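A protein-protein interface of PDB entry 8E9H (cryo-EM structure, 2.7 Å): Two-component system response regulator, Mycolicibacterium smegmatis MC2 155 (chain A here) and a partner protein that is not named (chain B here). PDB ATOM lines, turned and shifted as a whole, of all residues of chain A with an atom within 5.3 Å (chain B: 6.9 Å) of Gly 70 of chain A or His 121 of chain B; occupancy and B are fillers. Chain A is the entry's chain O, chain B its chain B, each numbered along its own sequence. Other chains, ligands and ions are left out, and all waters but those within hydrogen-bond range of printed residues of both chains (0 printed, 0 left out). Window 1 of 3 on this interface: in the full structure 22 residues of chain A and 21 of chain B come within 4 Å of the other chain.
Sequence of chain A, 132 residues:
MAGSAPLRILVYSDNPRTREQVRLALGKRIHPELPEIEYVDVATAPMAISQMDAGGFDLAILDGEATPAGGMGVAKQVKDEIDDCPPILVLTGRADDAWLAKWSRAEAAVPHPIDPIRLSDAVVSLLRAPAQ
The side-chain hydroxyl (OH) of Tyr 128 of chain B lies within hydrogen-bond range of the backbone carbonyl oxygen (O) of Thr 67 of chain A. The backbone carbonyl oxygen (O) of Pro 68 of chain A lies within hydrogen-bond range of the backbone NH (N) of Val 125 of chain B, 3.2 Å away. O of Gly 73 of chain A lies within hydrogen-bond range of NH1 of Arg 85 of chain B, at 3.4 Å. N of Gly 73 of chain A sits at hydrogen-bond distance from O of His 121 of chain B. The backbone carbonyl oxygen (O) of Thr 67 of chain A lies close to the side-chain carboxylate (OD2) of Asp 120 of chain B (2.8 Å). N of Gly 70 of chain A lies close to O of Asp 120 of chain B (2.4 Å).
OH of Tyr 12 of chain A lies within hydrogen-bond range of O of Ala 69 of chain A, at 2.5 Å. The guanidinium group (NH1) of Arg 85 of chain B is in hydrogen-bond range of the backbone carbonyl oxygen (O) of Val 122 of chain B, 2.8 Å away. The backbone carbonyl oxygen (O) of Gln 117 of chain B lies close to a ring nitrogen (ND1) of His 121 of chain B. OD1 of Asp 120 of chain B sits at hydrogen-bond distance from ND1 of His 121 of chain B (3.0 Å). The side-chain carboxylate of Asp 120 of chain B lies within hydrogen-bond range of the side-chain hydroxyl of Tyr 128 of chain B (2.8 Å).
Gly 64 of chain A touches His 121 of chain B (O to CD2, 3.8 Å). Pro 68 of chain A touches Asp 120 of chain B. O of Pro 68 of chain A touches CA of Pro 124 of chain B (3.7 Å). CA of Pro 68 of chain A touches OH of Tyr 128 of chain B, 3.6 Å away. Ala 69 of chain A touches Asp 120 of chain B. Gly 70 of chain A touches His 121 of chain B (CA to CA, 3.96 Å). Met 72 of chain A touches His 121 of chain B (CB to O, 3.8 Å). Val 122 of chain B touches Gly 73 of chain A (O to CA, 3.4 Å).
Gly 70 of chain A touches two residues of chain B. Of chain A, only Gly 64 (3.8 Å), Gly 70 (3.96 Å), Met 72 (3.8 Å) and Gly 73 (3.3 Å) come within 4 Å of His 121 of chain B. Of the printed residues of chain B, Gly 73 of chain A touches Arg 85 (3.4 Å), His 121 (3.3 Å) and Val 122 (3.4 Å). Of the printed residues of chain A, Asp 120 of chain B touches Thr 67, Pro 68, Ala 69 and Gly 70. Of the printed residues of chain B, Pro 68 of chain A touches Asp 120, Pro 124, Val 125 and Tyr 128. Val 116 of chain B touches none of the printed residues of chain A. The nearest residue of chain B that does not touch Gly 70 of chain A is Val 122 of chain B (4.9 Å). The nearest residue of chain A that does not touch His 121 of chain B is Asp 97 of chain A (4.4 Å). The nearest printed residue of chain B that does not touch Met 72 of chain A is Val 122 of chain B (5.2 Å).
Hydrophobic or aromatic side chains of chain B that line the printed part of chain A: His 121 and Tyr 128. Of the 14 printed residues of chain A, 7 touch a printed residue of chain B. Hydrophobic or aromatic side chains of chain A within 4 Å of the printed part of chain B: Met 72. Among the printed residues, 14 pairs touch across the chains. Among the printed residues, no Asp or Glu carboxylate lies within 4 Å of a Lys or Arg side-chain nitrogen of the other chain.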
ATOM      1  N   TYR A  12       8.961   6.110 -11.733  1.00  0.00           N
ATOM      2  CA  TYR A  12      10.000   5.533 -10.894  1.00  0.00           C
ATOM      3  C   TYR A  12      11.010   6.610 -10.534  1.00  0.00           C
ATOM      4  O   TYR A  12      11.626   7.211 -11.419  1.00  0.00           O
ATOM      5  CB  TYR A  12      10.696   4.379 -11.608  1.00  0.00           C
ATOM      6  CG  TYR A  12      11.981   3.959 -10.945  1.00  0.00           C
ATOM      7  CD1 TYR A  12      11.985   3.465  -9.655  1.00  0.00           C
ATOM      8  CD2 TYR A  12      13.189   4.067 -11.607  1.00  0.00           C
ATOM      9  CE1 TYR A  12      13.155   3.085  -9.045  1.00  0.00           C
ATOM     10  CE2 TYR A  12      14.363   3.692 -11.005  1.00  0.00           C
ATOM     11  CZ  TYR A  12      14.342   3.201  -9.724  1.00  0.00           C
ATOM     12  OH  TYR A  12      15.515   2.824  -9.118  1.00  0.00           O
ATOM     13  N   ASP A  63      13.490   7.835 -13.512  1.00  0.00           N
ATOM     14  CA  ASP A  63      14.409   8.907 -13.152  1.00  0.00           C
ATOM     15  C   ASP A  63      15.836   8.407 -13.312  1.00  0.00           C
ATOM     16  O   ASP A  63      16.266   7.496 -12.599  1.00  0.00           O
ATOM     17  CB  ASP A  63      14.150   9.372 -11.724  1.00  0.00           C
ATOM     18  CG  ASP A  63      14.999  10.563 -11.341  1.00  0.00           C
ATOM     19  OD1 ASP A  63      15.728  11.079 -12.212  1.00  0.00           O
ATOM     20  OD2 ASP A  63      14.941  10.983 -10.167  1.00  0.00           O
ATOM     21  N   GLY A  64      16.577   9.003 -14.241  1.00  0.00           N
ATOM     22  CA  GLY A  64      17.954   8.598 -14.439  1.00  0.00           C
ATOM     23  C   GLY A  64      18.823   8.856 -13.227  1.00  0.00           C
ATOM     24  O   GLY A  64      19.911   8.290 -13.108  1.00  0.00           O
ATOM     25  N   GLU A  65      18.363   9.708 -12.318  1.00  0.00           N
ATOM     26  CA  GLU A  65      19.120  10.064 -11.127  1.00  0.00           C
ATOM     27  C   GLU A  65      18.751   9.222  -9.913  1.00  0.00           C
ATOM     28  O   GLU A  65      19.200   9.535  -8.806  1.00  0.00           O
ATOM     29  CB  GLU A  65      18.912  11.544 -10.800  1.00  0.00           C
ATOM     30  N   ALA A  66      17.949   8.174 -10.084  1.00  0.00           N
ATOM     31  CA  ALA A  66      17.557   7.345  -8.953  1.00  0.00           C
ATOM     32  C   ALA A  66      18.790   6.813  -8.237  1.00  0.00           C
ATOM     33  O   ALA A  66      19.739   6.344  -8.870  1.00  0.00           O
ATOM     34  CB  ALA A  66      16.677   6.191  -9.426  1.00  0.00           C
ATOM     35  N   THR A  67      18.772   6.889  -6.905  1.00  0.00           N
ATOM     36  CA  THR A  67      19.983   6.623  -6.131  1.00  0.00           C
ATOM     37  C   THR A  67      20.405   5.163  -6.178  1.00  0.00           C
ATOM     38  O   THR A  67      21.460   4.861  -6.761  1.00  0.00           O
ATOM     39  CB  THR A  67      19.776   7.108  -4.694  1.00  0.00           C
ATOM     40  OG1 THR A  67      19.745   8.541  -4.669  1.00  0.00           O
ATOM     41  CG2 THR A  67      20.886   6.602  -3.785  1.00  0.00           C
ATOM     42  N   PRO A  68      19.657   4.216  -5.603  1.00  0.00           N
ATOM     43  CA  PRO A  68      20.145   2.831  -5.569  1.00  0.00           C
ATOM     44  C   PRO A  68      20.215   2.172  -6.931  1.00  0.00           C
ATOM     45  O   PRO A  68      21.048   1.277  -7.120  1.00  0.00           O
ATOM     46  CB  PRO A  68      19.124   2.127  -4.672  1.00  0.00           C
ATOM     47  CG  PRO A  68      17.872   2.874  -4.919  1.00  0.00           C
ATOM     48  CD  PRO A  68      18.283   4.314  -5.084  1.00  0.00           C
ATOM     49  N   ALA A  69      19.377   2.582  -7.882  1.00  0.00           N
ATOM     50  CA  ALA A  69      19.384   1.982  -9.214  1.00  0.00           C
ATOM     51  C   ALA A  69      18.880   3.043 -10.189  1.00  0.00           C
ATOM     52  O   ALA A  69      17.683   3.333 -10.224  1.00  0.00           O
ATOM     53  CB  ALA A  69      18.527   0.731  -9.258  1.00  0.00           C
ATOM     54  N   GLY A  70      19.795   3.594 -10.980  1.00  0.00           N
ATOM     55  CA  GLY A  70      19.442   4.691 -11.852  1.00  0.00           C
ATOM     56  C   GLY A  70      18.407   4.291 -12.885  1.00  0.00           C
ATOM     57  O   GLY A  70      18.256   3.123 -13.235  1.00  0.00           O
ATOM     58  N   GLY A  71      17.685   5.295 -13.379  1.00  0.00           N
ATOM     59  CA  GLY A  71      16.611   5.046 -14.318  1.00  0.00           C
ATOM     60  C   GLY A  71      17.060   4.444 -15.631  1.00  0.00           C
ATOM     61  O   GLY A  71      16.332   3.636 -16.206  1.00  0.00           O
ATOM     62  N   MET A  72      18.232   4.831 -16.131  1.00  0.00           N
ATOM     63  CA  MET A  72      18.696   4.293 -17.406  1.00  0.00           C
ATOM     64  C   MET A  72      18.939   2.794 -17.311  1.00  0.00           C
ATOM     65  O   MET A  72      18.602   2.040 -18.234  1.00  0.00           O
ATOM     66  CB  MET A  72      19.963   5.019 -17.839  1.00  0.00           C
ATOM     67  CG  MET A  72      19.793   6.518 -17.886  1.00  0.00           C
ATOM     68  SD  MET A  72      21.140   7.365 -18.715  1.00  0.00           S
ATOM     69  CE  MET A  72      21.543   8.606 -17.495  1.00  0.00           C
ATOM     70  N   GLY A  73      19.527   2.341 -16.206  1.00  0.00           N
ATOM     71  CA  GLY A  73      19.700   0.915 -16.017  1.00  0.00           C
ATOM     72  C   GLY A  73      18.373   0.184 -15.992  1.00  0.00           C
ATOM     73  O   GLY A  73      18.229  -0.885 -16.584  1.00  0.00           O
ATOM     74  N   VAL A  74      17.380   0.764 -15.318  1.00  0.00           N
ATOM     75  CA  VAL A  74      16.065   0.138 -15.263  1.00  0.00           C
ATOM     76  C   VAL A  74      15.434   0.104 -16.646  1.00  0.00           C
ATOM     77  O   VAL A  74      14.751  -0.858 -17.005  1.00  0.00           O
ATOM     78  CB  VAL A  74      15.166   0.869 -14.253  1.00  0.00           C
ATOM     79  CG1 VAL A  74      13.785   0.256 -14.244  1.00  0.00           C
ATOM     80  CG2 VAL A  74      15.775   0.808 -12.871  1.00  0.00           C
ATOM     81  N   ASP A  97      24.503  13.141 -20.110  1.00  0.00           N
ATOM     82  CA  ASP A  97      23.848  11.850 -19.974  1.00  0.00           C
ATOM     83  C   ASP A  97      23.061  11.465 -21.214  1.00  0.00           C
ATOM     84  O   ASP A  97      22.666  10.301 -21.343  1.00  0.00           O
ATOM     85  CB  ASP A  97      22.910  11.855 -18.764  1.00  0.00           C
ATOM     86  CG  ASP A  97      23.599  11.417 -17.487  1.00  0.00           C
ATOM     87  OD1 ASP A  97      24.641  10.733 -17.566  1.00  0.00           O
ATOM     88  OD2 ASP A  97      23.095  11.753 -16.396  1.00  0.00           O
ATOM     89  N   ARG B  85      27.058  -2.786 -18.035  1.00  0.00           N
ATOM     90  CA  ARG B  85      25.697  -3.298 -17.959  1.00  0.00           C
ATOM     91  C   ARG B  85      25.587  -4.651 -18.640  1.00  0.00           C
ATOM     92  O   ARG B  85      24.869  -5.534 -18.164  1.00  0.00           O
ATOM     93  CB  ARG B  85      24.717  -2.311 -18.584  1.00  0.00           C
ATOM     94  CG  ARG B  85      23.272  -2.789 -18.572  1.00  0.00           C
ATOM     95  CD  ARG B  85      22.664  -2.683 -17.196  1.00  0.00           C
ATOM     96  NE  ARG B  85      21.679  -3.728 -16.958  1.00  0.00           N
ATOM     97  CZ  ARG B  85      20.790  -3.709 -15.976  1.00  0.00           C
ATOM     98  NH1 ARG B  85      20.732  -2.707 -15.116  1.00  0.00           N
ATOM     99  NH2 ARG B  85      19.939  -4.721 -15.852  1.00  0.00           N
ATOM    100  N   ALA B 104      33.389   4.592  -8.580  1.00  0.00           N
ATOM    101  CA  ALA B 104      32.320   3.651  -8.888  1.00  0.00           C
ATOM    102  C   ALA B 104      31.029   4.050  -8.194  1.00  0.00           C
ATOM    103  O   ALA B 104      29.945   3.951  -8.775  1.00  0.00           O
ATOM    104  CB  ALA B 104      32.731   2.241  -8.477  1.00  0.00           C
ATOM    105  N   SER B 105      31.125   4.504  -6.949  1.00  0.00           N
ATOM    106  CA  SER B 105      29.930   4.809  -6.176  1.00  0.00           C
ATOM    107  C   SER B 105      29.243   6.089  -6.633  1.00  0.00           C
ATOM    108  O   SER B 105      28.020   6.100  -6.793  1.00  0.00           O
ATOM    109  CB  SER B 105      30.292   4.909  -4.700  1.00  0.00           C
ATOM    110  OG  SER B 105      31.300   5.878  -4.507  1.00  0.00           O
ATOM    111  N   VAL B 116      30.495   8.372 -15.429  1.00  0.00           N
ATOM    112  CA  VAL B 116      29.055   8.145 -15.312  1.00  0.00           C
ATOM    113  C   VAL B 116      28.461   8.717 -14.038  1.00  0.00           C
ATOM    114  O   VAL B 116      27.233   8.787 -13.920  1.00  0.00           O
ATOM    115  CB  VAL B 116      28.767   6.634 -15.400  1.00  0.00           C
ATOM    116  CG1 VAL B 116      27.311   6.341 -15.116  1.00  0.00           C
ATOM    117  CG2 VAL B 116      29.142   6.113 -16.766  1.00  0.00           C
ATOM    118  N   GLN B 117      29.286   9.147 -13.087  1.00  0.00           N
ATOM    119  CA  GLN B 117      28.796   9.703 -11.828  1.00  0.00           C
ATOM    120  C   GLN B 117      28.038   8.652 -11.027  1.00  0.00           C
ATOM    121  O   GLN B 117      26.901   8.863 -10.607  1.00  0.00           O
ATOM    122  CB  GLN B 117      27.920  10.933 -12.065  1.00  0.00           C
ATOM    123  CG  GLN B 117      28.619  12.047 -12.806  1.00  0.00           C
ATOM    124  CD  GLN B 117      29.970  12.365 -12.216  1.00  0.00           C
ATOM    125  OE1 GLN B 117      30.085  12.655 -11.028  1.00  0.00           O
ATOM    126  NE2 GLN B 117      31.004  12.298 -13.040  1.00  0.00           N
ATOM    127  N   GLY B 118      28.678   7.508 -10.819  1.00  0.00           N
ATOM    128  CA  GLY B 118      28.099   6.452 -10.021  1.00  0.00           C
ATOM    129  C   GLY B 118      27.676   5.262 -10.850  1.00  0.00           C
ATOM    130  O   GLY B 118      26.992   5.408 -11.864  1.00  0.00           O
ATOM    131  N   VAL B 119      28.082   4.070 -10.419  1.00  0.00           N
ATOM    132  CA  VAL B 119      27.687   2.853 -11.116  1.00  0.00           C
ATOM    133  C   VAL B 119      26.179   2.713 -11.124  1.00  0.00           C
ATOM    134  O   VAL B 119      25.591   2.278 -12.118  1.00  0.00           O
ATOM    135  CB  VAL B 119      28.351   1.633 -10.456  1.00  0.00           C
ATOM    136  CG1 VAL B 119      27.654   0.363 -10.873  1.00  0.00           C
ATOM    137  CG2 VAL B 119      29.805   1.581 -10.820  1.00  0.00           C
ATOM    138  N   ASP B 120      25.528   3.074 -10.020  1.00  0.00           N
ATOM    139  CA  ASP B 120      24.096   2.851  -9.893  1.00  0.00           C
ATOM    140  C   ASP B 120      23.307   3.470 -11.033  1.00  0.00           C
ATOM    141  O   ASP B 120      22.133   3.136 -11.211  1.00  0.00           O
ATOM    142  CB  ASP B 120      23.610   3.396  -8.556  1.00  0.00           C
ATOM    143  CG  ASP B 120      23.992   4.836  -8.350  1.00  0.00           C
ATOM    144  OD1 ASP B 120      24.101   5.571  -9.351  1.00  0.00           O
ATOM    145  OD2 ASP B 120      24.193   5.237  -7.185  1.00  0.00           O
ATOM    146  N   HIS B 121      23.917   4.359 -11.814  1.00  0.00           N
ATOM    147  CA  HIS B 121      23.233   4.888 -12.983  1.00  0.00           C
ATOM    148  C   HIS B 121      22.930   3.808 -14.009  1.00  0.00           C
ATOM    149  O   HIS B 121      22.060   4.013 -14.861  1.00  0.00           O
ATOM    150  CB  HIS B 121      24.067   5.989 -13.632  1.00  0.00           C
ATOM    151  CG  HIS B 121      23.911   7.323 -12.977  1.00  0.00           C
ATOM    152  ND1 HIS B 121      23.918   7.484 -11.610  1.00  0.00           N
ATOM    153  CD2 HIS B 121      23.727   8.556 -13.500  1.00  0.00           C
ATOM    154  CE1 HIS B 121      23.755   8.760 -11.318  1.00  0.00           C
ATOM    155  NE2 HIS B 121      23.636   9.433 -12.447  1.00  0.00           N
ATOM    156  N   VAL B 122      23.620   2.670 -13.954  1.00  0.00           N
ATOM    157  CA  VAL B 122      23.418   1.617 -14.944  1.00  0.00           C
ATOM    158  C   VAL B 122      23.129   0.256 -14.335  1.00  0.00           C
ATOM    159  O   VAL B 122      22.527  -0.595 -15.012  1.00  0.00           O
ATOM    160  CB  VAL B 122      24.637   1.528 -15.883  1.00  0.00           C
ATOM    161  CG1 VAL B 122      24.817   2.833 -16.618  1.00  0.00           C
ATOM    162  CG2 VAL B 122      25.887   1.183 -15.106  1.00  0.00           C
ATOM    163  N   VAL B 123      23.521  -0.028 -13.096  1.00  0.00           N
ATOM    164  CA  VAL B 123      23.214  -1.319 -12.479  1.00  0.00           C
ATOM    165  C   VAL B 123      22.893  -1.108 -11.014  1.00  0.00           C
ATOM    166  O   VAL B 123      23.457  -0.230 -10.352  1.00  0.00           O
ATOM    167  CB  VAL B 123      24.385  -2.311 -12.609  1.00  0.00           C
ATOM    168  CG1 VAL B 123      24.595  -2.691 -14.054  1.00  0.00           C
ATOM    169  CG2 VAL B 123      25.646  -1.715 -12.043  1.00  0.00           C
ATOM    170  N   PRO B 124      21.992  -1.925 -10.468  1.00  0.00           N
ATOM    171  CA  PRO B 124      21.667  -1.794  -9.043  1.00  0.00           C
ATOM    172  C   PRO B 124      22.902  -2.027  -8.190  1.00  0.00           C
ATOM    173  O   PRO B 124      23.609  -3.022  -8.358  1.00  0.00           O
ATOM    174  CB  PRO B 124      20.610  -2.879  -8.813  1.00  0.00           C
ATOM    175  CG  PRO B 124      20.097  -3.210 -10.157  1.00  0.00           C
ATOM    176  CD  PRO B 124      21.241  -3.026 -11.088  1.00  0.00           C
ATOM    177  N   VAL B 125      23.153  -1.110  -7.264  1.00  0.00           N
ATOM    178  CA  VAL B 125      24.300  -1.185  -6.373  1.00  0.00           C
ATOM    179  C   VAL B 125      23.809  -1.608  -5.000  1.00  0.00           C
ATOM    180  O   VAL B 125      22.853  -1.033  -4.469  1.00  0.00           O
ATOM    181  CB  VAL B 125      25.043   0.157  -6.303  1.00  0.00           C
ATOM    182  CG1 VAL B 125      26.126   0.099  -5.251  1.00  0.00           C
ATOM    183  CG2 VAL B 125      25.632   0.498  -7.653  1.00  0.00           C
ATOM    184  N   TYR B 128      27.870   0.605  -1.175  1.00  0.00           N
ATOM    185  CA  TYR B 128      28.759   1.679  -1.590  1.00  0.00           C
ATOM    186  C   TYR B 128      29.981   1.674  -0.688  1.00  0.00           C
ATOM    187  O   TYR B 128      29.852   1.573   0.535  1.00  0.00           O
ATOM    188  CB  TYR B 128      28.062   3.033  -1.511  1.00  0.00           C
ATOM    189  CG  TYR B 128      26.886   3.177  -2.435  1.00  0.00           C
ATOM    190  CD1 TYR B 128      27.052   3.653  -3.722  1.00  0.00           C
ATOM    191  CD2 TYR B 128      25.612   2.839  -2.024  1.00  0.00           C
ATOM    192  CE1 TYR B 128      25.985   3.790  -4.568  1.00  0.00           C
ATOM    193  CE2 TYR B 128      24.538   2.972  -2.865  1.00  0.00           C
ATOM    194  CZ  TYR B 128      24.730   3.448  -4.137  1.00  0.00           C
ATOM    195  OH  TYR B 128      23.659   3.585  -4.983  1.00  0.00           O
